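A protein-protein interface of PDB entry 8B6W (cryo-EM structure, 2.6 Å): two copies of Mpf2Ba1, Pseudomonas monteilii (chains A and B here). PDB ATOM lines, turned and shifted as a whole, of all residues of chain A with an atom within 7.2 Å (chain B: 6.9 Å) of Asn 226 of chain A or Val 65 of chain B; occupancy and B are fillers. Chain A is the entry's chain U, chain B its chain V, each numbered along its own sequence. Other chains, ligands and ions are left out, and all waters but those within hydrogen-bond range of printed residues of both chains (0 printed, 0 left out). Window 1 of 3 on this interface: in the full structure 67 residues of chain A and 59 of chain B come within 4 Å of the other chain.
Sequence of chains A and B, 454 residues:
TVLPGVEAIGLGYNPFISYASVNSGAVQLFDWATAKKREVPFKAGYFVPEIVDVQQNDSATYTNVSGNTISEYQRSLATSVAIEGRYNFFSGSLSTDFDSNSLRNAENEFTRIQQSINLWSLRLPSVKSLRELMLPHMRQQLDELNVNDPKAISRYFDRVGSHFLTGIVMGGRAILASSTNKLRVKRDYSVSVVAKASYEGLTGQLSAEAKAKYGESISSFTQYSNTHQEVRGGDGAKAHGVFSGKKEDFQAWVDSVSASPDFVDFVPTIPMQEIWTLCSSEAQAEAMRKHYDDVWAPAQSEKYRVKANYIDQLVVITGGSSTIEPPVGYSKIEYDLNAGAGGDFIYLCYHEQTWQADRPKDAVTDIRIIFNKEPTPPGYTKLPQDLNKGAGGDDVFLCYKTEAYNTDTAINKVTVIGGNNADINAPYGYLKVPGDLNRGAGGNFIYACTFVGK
OH of Tyr 224 of chain A touches CG1 of Val 65 of chain B, 3.8 Å away.
Tyr 224 of chain A touches Ser 66 of chain B.
Val 65 of chain B touches Ser 225 of chain A (CA to O, 3.5 Å).
CA of Asn 226 of chain A touches O of Asn 64 of chain B (3.5 Å).
Asn 226 of chain A touches Val 65 of chain B (ND2 to CG2, 3.7 Å).
CA of Thr 63 of chain B touches O of Thr 227 of chain A, at 3.5 Å.
Tyr 62 of chain B touches His 228 of chain A (O to CA, 3.5 Å).
His 228 of chain A touches Thr 63 of chain B (CD2 to OG1, 3.5 Å).
Position printed for both chains: 111.
Of the printed residues of chain B, Tyr 224 of chain A touches Val 65 (3.8 Å) and Ser 66 (3.5 Å).
Printed residues of chain B within 4 Å of Ser 225 of chain A: Val 65 and Ser 66.
Asn 226 of chain A touches just these residues of chain B: Asn 64 and Val 65.
Printed residues of chain A within 4 Å of Asn 64 of chain B: Asn 226 and Thr 227.
Printed residues of chain A within 4 Å of Val 65 of chain B: Tyr 224, Ser 225 and Asn 226.
Printed residues of chain A within 4 Å of Ser 66 of chain B: Tyr 224 (3.5 Å) and Ser 225 (2.9 Å).
Gln 114 of chain B touches none of the printed residues of chain A.
The nearest residue of chain A that does not touch Val 65 of chain B is Thr 227 of chain A (5.0 Å).
Of the 12 printed residues of chain A, 5 touch a printed residue of chain B.
Printed residues of chain A that touch a printed residue of chain B: Tyr 224, Ser 225, Asn 226, Thr 227 and His 228.
Along chain A the printed residues that touch a printed residue of chain B span positions 224 to 228.
Of the 11 printed residues of chain B, 5 touch a printed residue of chain A.
Hydrophobic or aromatic side chains of chain B that line the printed part of chain A: Val 65.
Among the printed residues, no Asp or Glu carboxylate lies within 4 Å of a Lys or Arg side-chain nitrogen of the other chain.
The backbone carbonyl oxygen (O) of Ala 177 of chain A sits at hydrogen-bond distance from the backbone NH (N) of His 228 of chain A (2.8 Å).
The backbone NH of Ser 179 of chain A is in hydrogen-bond range of the backbone carbonyl oxygen of Asn 226 of chain A (2.8 Å).
The backbone NH (N) of Asn 181 of chain A lies within hydrogen-bond range of the backbone carbonyl oxygen (O) of Tyr 224 of chain A, 3.0 Å away.
The side-chain hydroxyl of Tyr 62 of chain B sits at hydrogen-bond distance from the side-chain amide nitrogen of Asn 64 of chain B (3.4 Å).
N of Thr 63 of chain B sits at hydrogen-bond distance from O of Gln 114 of chain B (2.9 Å).
The backbone NH (N) of Arg 112 of chain B lies within hydrogen-bond range of the backbone carbonyl oxygen (O) of Val 65 of chain B (2.7 Å).
N of Ser 225 of chain A lies within hydrogen-bond range of O of Ser 66 of chain B (2.9 Å).
The backbone NH of Thr 227 of chain A is in hydrogen-bond range of the backbone carbonyl oxygen of Asn 64 of chain B (2.8 Å).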
ATOM      1  N   GLU A 109      -0.249 -24.770  -4.284  1.00  0.00           N
ATOM      2  CA  GLU A 109      -0.831 -26.078  -4.522  1.00  0.00           C
ATOM      3  C   GLU A 109      -2.335 -25.982  -4.367  1.00  0.00           C
ATOM      4  O   GLU A 109      -2.830 -25.236  -3.519  1.00  0.00           O
ATOM      5  CB  GLU A 109      -0.262 -27.106  -3.552  1.00  0.00           C
ATOM      6  CG  GLU A 109      -0.689 -28.517  -3.833  1.00  0.00           C
ATOM      7  CD  GLU A 109       0.163 -29.521  -3.094  1.00  0.00           C
ATOM      8  OE1 GLU A 109       0.003 -30.734  -3.336  1.00  0.00           O
ATOM      9  OE2 GLU A 109       0.995 -29.094  -2.268  1.00  0.00           O
ATOM     10  N   THR A 111      -6.023 -28.628  -4.849  1.00  0.00           N
ATOM     11  CA  THR A 111      -6.693 -29.861  -5.223  1.00  0.00           C
ATOM     12  C   THR A 111      -8.189 -29.635  -5.161  1.00  0.00           C
ATOM     13  O   THR A 111      -8.679 -28.935  -4.275  1.00  0.00           O
ATOM     14  CB  THR A 111      -6.311 -31.014  -4.295  1.00  0.00           C
ATOM     15  OG1 THR A 111      -4.927 -31.333  -4.470  1.00  0.00           O
ATOM     16  CG2 THR A 111      -7.147 -32.232  -4.594  1.00  0.00           C
ATOM     17  N   ALA A 177     -12.068 -29.471  -1.363  1.00  0.00           N
ATOM     18  CA  ALA A 177     -11.240 -28.431  -1.945  1.00  0.00           C
ATOM     19  C   ALA A 177     -10.098 -28.139  -0.992  1.00  0.00           C
ATOM     20  O   ALA A 177     -10.297 -28.064   0.220  1.00  0.00           O
ATOM     21  CB  ALA A 177     -12.040 -27.158  -2.216  1.00  0.00           C
ATOM     22  N   SER A 178      -8.901 -27.988  -1.538  1.00  0.00           N
ATOM     23  CA  SER A 178      -7.716 -27.784  -0.727  1.00  0.00           C
ATOM     24  C   SER A 178      -6.777 -26.835  -1.447  1.00  0.00           C
ATOM     25  O   SER A 178      -6.693 -26.846  -2.675  1.00  0.00           O
ATOM     26  CB  SER A 178      -7.010 -29.110  -0.447  1.00  0.00           C
ATOM     27  OG  SER A 178      -5.796 -28.898   0.241  1.00  0.00           O
ATOM     28  N   SER A 179      -6.096 -25.998  -0.675  1.00  0.00           N
ATOM     29  CA  SER A 179      -5.169 -25.013  -1.199  1.00  0.00           C
ATOM     30  C   SER A 179      -3.974 -24.949  -0.267  1.00  0.00           C
ATOM     31  O   SER A 179      -4.118 -25.128   0.943  1.00  0.00           O
ATOM     32  CB  SER A 179      -5.817 -23.633  -1.321  1.00  0.00           C
ATOM     33  OG  SER A 179      -7.038 -23.715  -2.030  1.00  0.00           O
ATOM     34  N   THR A 180      -2.794 -24.725  -0.827  1.00  0.00           N
ATOM     35  CA  THR A 180      -1.641 -24.366  -0.020  1.00  0.00           C
ATOM     36  C   THR A 180      -0.829 -23.302  -0.735  1.00  0.00           C
ATOM     37  O   THR A 180      -0.694 -23.329  -1.960  1.00  0.00           O
ATOM     38  CB  THR A 180      -0.761 -25.583   0.263  1.00  0.00           C
ATOM     39  OG1 THR A 180      -1.514 -26.558   0.991  1.00  0.00           O
ATOM     40  CG2 THR A 180       0.454 -25.181   1.072  1.00  0.00           C
ATOM     41  N   ASN A 181      -0.310 -22.358   0.035  1.00  0.00           N
ATOM     42  CA  ASN A 181       0.687 -21.414  -0.437  1.00  0.00           C
ATOM     43  C   ASN A 181       1.871 -21.445   0.508  1.00  0.00           C
ATOM     44  O   ASN A 181       1.700 -21.538   1.723  1.00  0.00           O
ATOM     45  CB  ASN A 181       0.130 -19.997  -0.509  1.00  0.00           C
ATOM     46  CG  ASN A 181      -1.141 -19.915  -1.312  1.00  0.00           C
ATOM     47  OD1 ASN A 181      -2.237 -19.943  -0.761  1.00  0.00           O
ATOM     48  ND2 ASN A 181      -1.003 -19.795  -2.622  1.00  0.00           N
ATOM     49  N   TYR A 224       0.377 -20.852   4.306  1.00  0.00           N
ATOM     50  CA  TYR A 224      -1.056 -20.755   4.491  1.00  0.00           C
ATOM     51  C   TYR A 224      -1.690 -21.999   3.900  1.00  0.00           C
ATOM     52  O   TYR A 224      -1.309 -22.438   2.816  1.00  0.00           O
ATOM     53  CB  TYR A 224      -1.606 -19.494   3.822  1.00  0.00           C
ATOM     54  CG  TYR A 224      -3.105 -19.378   3.848  1.00  0.00           C
ATOM     55  CD1 TYR A 224      -3.754 -18.819   4.937  1.00  0.00           C
ATOM     56  CD2 TYR A 224      -3.871 -19.823   2.785  1.00  0.00           C
ATOM     57  CE1 TYR A 224      -5.129 -18.718   4.971  1.00  0.00           C
ATOM     58  CE2 TYR A 224      -5.246 -19.718   2.806  1.00  0.00           C
ATOM     59  CZ  TYR A 224      -5.871 -19.166   3.904  1.00  0.00           C
ATOM     60  OH  TYR A 224      -7.242 -19.048   3.922  1.00  0.00           O
ATOM     61  N   SER A 225      -2.642 -22.571   4.620  1.00  0.00           N
ATOM     62  CA  SER A 225      -3.374 -23.735   4.152  1.00  0.00           C
ATOM     63  C   SER A 225      -4.860 -23.475   4.284  1.00  0.00           C
ATOM     64  O   SER A 225      -5.301 -22.803   5.218  1.00  0.00           O
ATOM     65  CB  SER A 225      -3.002 -24.992   4.934  1.00  0.00           C
ATOM     66  OG  SER A 225      -1.628 -25.291   4.789  1.00  0.00           O
ATOM     67  N   ASN A 226      -5.622 -23.987   3.335  1.00  0.00           N
ATOM     68  CA  ASN A 226      -7.067 -23.977   3.422  1.00  0.00           C
ATOM     69  C   ASN A 226      -7.566 -25.324   2.940  1.00  0.00           C
ATOM     70  O   ASN A 226      -7.056 -25.862   1.958  1.00  0.00           O
ATOM     71  CB  ASN A 226      -7.665 -22.851   2.585  1.00  0.00           C
ATOM     72  CG  ASN A 226      -9.125 -22.633   2.870  1.00  0.00           C
ATOM     73  OD1 ASN A 226      -9.928 -23.560   2.784  1.00  0.00           O
ATOM     74  ND2 ASN A 226      -9.482 -21.401   3.203  1.00  0.00           N
ATOM     75  N   THR A 227      -8.542 -25.876   3.644  1.00  0.00           N
ATOM     76  CA  THR A 227      -9.191 -27.100   3.212  1.00  0.00           C
ATOM     77  C   THR A 227     -10.669 -27.009   3.531  1.00  0.00           C
ATOM     78  O   THR A 227     -11.060 -26.422   4.539  1.00  0.00           O
ATOM     79  CB  THR A 227      -8.585 -28.339   3.876  1.00  0.00           C
ATOM     80  OG1 THR A 227      -9.282 -29.507   3.430  1.00  0.00           O
ATOM     81  CG2 THR A 227      -8.684 -28.250   5.372  1.00  0.00           C
ATOM     82  N   HIS A 228     -11.485 -27.567   2.651  1.00  0.00           N
ATOM     83  CA  HIS A 228     -12.923 -27.578   2.832  1.00  0.00           C
ATOM     84  C   HIS A 228     -13.438 -28.916   2.336  1.00  0.00           C
ATOM     85  O   HIS A 228     -13.152 -29.307   1.205  1.00  0.00           O
ATOM     86  CB  HIS A 228     -13.582 -26.434   2.067  1.00  0.00           C
ATOM     87  CG  HIS A 228     -15.055 -26.339   2.285  1.00  0.00           C
ATOM     88  ND1 HIS A 228     -15.943 -27.255   1.765  1.00  0.00           N
ATOM     89  CD2 HIS A 228     -15.800 -25.433   2.960  1.00  0.00           C
ATOM     90  CE1 HIS A 228     -17.172 -26.921   2.119  1.00  0.00           C
ATOM     91  NE2 HIS A 228     -17.111 -25.818   2.842  1.00  0.00           N
ATOM     92  N   TYR B  62     -16.660 -29.979   6.813  1.00  0.00           N
ATOM     93  CA  TYR B  62     -15.396 -29.797   7.502  1.00  0.00           C
ATOM     94  C   TYR B  62     -14.713 -28.576   6.915  1.00  0.00           C
ATOM     95  O   TYR B  62     -14.840 -28.301   5.720  1.00  0.00           O
ATOM     96  CB  TYR B  62     -14.525 -31.032   7.346  1.00  0.00           C
ATOM     97  CG  TYR B  62     -13.183 -30.956   8.008  1.00  0.00           C
ATOM     98  CD1 TYR B  62     -13.018 -31.356   9.318  1.00  0.00           C
ATOM     99  CD2 TYR B  62     -12.070 -30.525   7.312  1.00  0.00           C
ATOM    100  CE1 TYR B  62     -11.799 -31.266   9.937  1.00  0.00           C
ATOM    101  CE2 TYR B  62     -10.838 -30.465   7.914  1.00  0.00           C
ATOM    102  CZ  TYR B  62     -10.710 -30.827   9.230  1.00  0.00           C
ATOM    103  OH  TYR B  62      -9.473 -30.813   9.824  1.00  0.00           O
ATOM    104  N   THR B  63     -14.011 -27.833   7.755  1.00  0.00           N
ATOM    105  CA  THR B  63     -13.228 -26.701   7.292  1.00  0.00           C
ATOM    106  C   THR B  63     -11.978 -26.597   8.140  1.00  0.00           C
ATOM    107  O   THR B  63     -12.036 -26.766   9.355  1.00  0.00           O
ATOM    108  CB  THR B  63     -14.021 -25.400   7.376  1.00  0.00           C
ATOM    109  OG1 THR B  63     -15.049 -25.400   6.382  1.00  0.00           O
ATOM    110  CG2 THR B  63     -13.115 -24.215   7.157  1.00  0.00           C
ATOM    111  N   ASN B  64     -10.852 -26.328   7.496  1.00  0.00           N
ATOM    112  CA  ASN B  64      -9.606 -26.152   8.218  1.00  0.00           C
ATOM    113  C   ASN B  64      -8.807 -25.045   7.559  1.00  0.00           C
ATOM    114  O   ASN B  64      -8.549 -25.090   6.355  1.00  0.00           O
ATOM    115  CB  ASN B  64      -8.811 -27.457   8.235  1.00  0.00           C
ATOM    116  CG  ASN B  64      -7.521 -27.338   8.995  1.00  0.00           C
ATOM    117  OD1 ASN B  64      -6.934 -26.266   9.087  1.00  0.00           O
ATOM    118  ND2 ASN B  64      -7.059 -28.454   9.543  1.00  0.00           N
ATOM    119  N   VAL B  65      -8.417 -24.060   8.353  1.00  0.00           N
ATOM    120  CA  VAL B  65      -7.594 -22.946   7.910  1.00  0.00           C
ATOM    121  C   VAL B  65      -6.448 -22.815   8.894  1.00  0.00           C
ATOM    122  O   VAL B  65      -6.677 -22.781  10.107  1.00  0.00           O
ATOM    123  CB  VAL B  65      -8.392 -21.633   7.841  1.00  0.00           C
ATOM    124  CG1 VAL B  65      -7.499 -20.496   7.418  1.00  0.00           C
ATOM    125  CG2 VAL B  65      -9.563 -21.782   6.898  1.00  0.00           C
ATOM    126  N   SER B  66      -5.228 -22.736   8.391  1.00  0.00           N
ATOM    127  CA  SER B  66      -4.098 -22.495   9.271  1.00  0.00           C
ATOM    128  C   SER B  66      -3.072 -21.623   8.576  1.00  0.00           C
ATOM    129  O   SER B  66      -2.866 -21.727   7.366  1.00  0.00           O
ATOM    130  CB  SER B  66      -3.451 -23.810   9.713  1.00  0.00           C
ATOM    131  OG  SER B  66      -2.997 -24.554   8.605  1.00  0.00           O
ATOM    132  N   GLY B  67      -2.438 -20.769   9.354  1.00  0.00           N
ATOM    133  CA  GLY B  67      -1.375 -19.918   8.850  1.00  0.00           C
ATOM    134  C   GLY B  67      -0.160 -20.033   9.736  1.00  0.00           C
ATOM    135  O   GLY B  67      -0.275 -20.157  10.952  1.00  0.00           O
ATOM    136  N   PHE B 110      -1.555 -19.455  13.598  1.00  0.00           N
ATOM    137  CA  PHE B 110      -2.982 -19.470  13.862  1.00  0.00           C
ATOM    138  C   PHE B 110      -3.594 -20.682  13.183  1.00  0.00           C
ATOM    139  O   PHE B 110      -3.144 -21.109  12.121  1.00  0.00           O
ATOM    140  CB  PHE B 110      -3.653 -18.161  13.421  1.00  0.00           C
ATOM    141  CG  PHE B 110      -4.057 -18.125  11.981  1.00  0.00           C
ATOM    142  CD1 PHE B 110      -5.277 -18.637  11.575  1.00  0.00           C
ATOM    143  CD2 PHE B 110      -3.233 -17.545  11.033  1.00  0.00           C
ATOM    144  CE1 PHE B 110      -5.654 -18.590  10.249  1.00  0.00           C
ATOM    145  CE2 PHE B 110      -3.607 -17.496   9.708  1.00  0.00           C
ATOM    146  CZ  PHE B 110      -4.818 -18.021   9.314  1.00  0.00           C
ATOM    147  N   THR B 111      -4.611 -21.244  13.822  1.00  0.00           N
ATOM    148  CA  THR B 111      -5.418 -22.298  13.231  1.00  0.00           C
ATOM    149  C   THR B 111      -6.874 -22.019  13.538  1.00  0.00           C
ATOM    150  O   THR B 111      -7.205 -21.555  14.628  1.00  0.00           O
ATOM    151  CB  THR B 111      -5.034 -23.674  13.775  1.00  0.00           C
ATOM    152  OG1 THR B 111      -3.709 -24.005  13.350  1.00  0.00           O
ATOM    153  CG2 THR B 111      -5.995 -24.723  13.281  1.00  0.00           C
ATOM    154  N   ARG B 112      -7.739 -22.279  12.568  1.00  0.00           N
ATOM    155  CA  ARG B 112      -9.166 -22.384  12.816  1.00  0.00           C
ATOM    156  C   ARG B 112      -9.675 -23.661  12.176  1.00  0.00           C
ATOM    157  O   ARG B 112      -9.331 -23.962  11.032  1.00  0.00           O
ATOM    158  CB  ARG B 112      -9.908 -21.171  12.269  1.00  0.00           C
ATOM    159  CG  ARG B 112      -9.583 -19.903  13.015  1.00  0.00           C
ATOM    160  CD  ARG B 112     -10.538 -18.781  12.677  1.00  0.00           C
ATOM    161  NE  ARG B 112     -10.333 -17.628  13.547  1.00  0.00           N
ATOM    162  CZ  ARG B 112     -11.301 -16.938  14.140  1.00  0.00           C
ATOM    163  NH1 ARG B 112     -12.579 -17.213  13.934  1.00  0.00           N
ATOM    164  NH2 ARG B 112     -10.976 -15.933  14.949  1.00  0.00           N
ATOM    165  N   ILE B 113     -10.486 -24.405  12.908  1.00  0.00           N
ATOM    166  CA  ILE B 113     -11.130 -25.602  12.398  1.00  0.00           C
ATOM    167  C   ILE B 113     -12.606 -25.510  12.729  1.00  0.00           C
ATOM    168  O   ILE B 113     -12.980 -25.033  13.803  1.00  0.00           O
ATOM    169  CB  ILE B 113     -10.523 -26.885  12.991  1.00  0.00           C
ATOM    170  CG1 ILE B 113      -9.043 -26.973  12.635  1.00  0.00           C
ATOM    171  CG2 ILE B 113     -11.273 -28.100  12.490  1.00  0.00           C
ATOM    172  CD1 ILE B 113      -8.329 -28.117  13.296  1.00  0.00           C
ATOM    173  N   GLN B 114     -13.440 -25.941  11.804  1.00  0.00           N
ATOM    174  CA  GLN B 114     -14.844 -26.158  12.082  1.00  0.00           C
ATOM    175  C   GLN B 114     -15.229 -27.536  11.591  1.00  0.00           C
ATOM    176  O   GLN B 114     -14.819 -27.959  10.512  1.00  0.00           O
ATOM    177  CB  GLN B 114     -15.714 -25.101  11.430  1.00  0.00           C
ATOM    178  CG  GLN B 114     -15.354 -23.705  11.858  1.00  0.00           C
ATOM    179  CD  GLN B 114     -16.398 -22.697  11.453  1.00  0.00           C
ATOM    180  OE1 GLN B 114     -17.317 -23.008  10.699  1.00  0.00           O
ATOM    181  NE2 GLN B 114     -16.270 -21.478  11.959  1.00  0.00           N
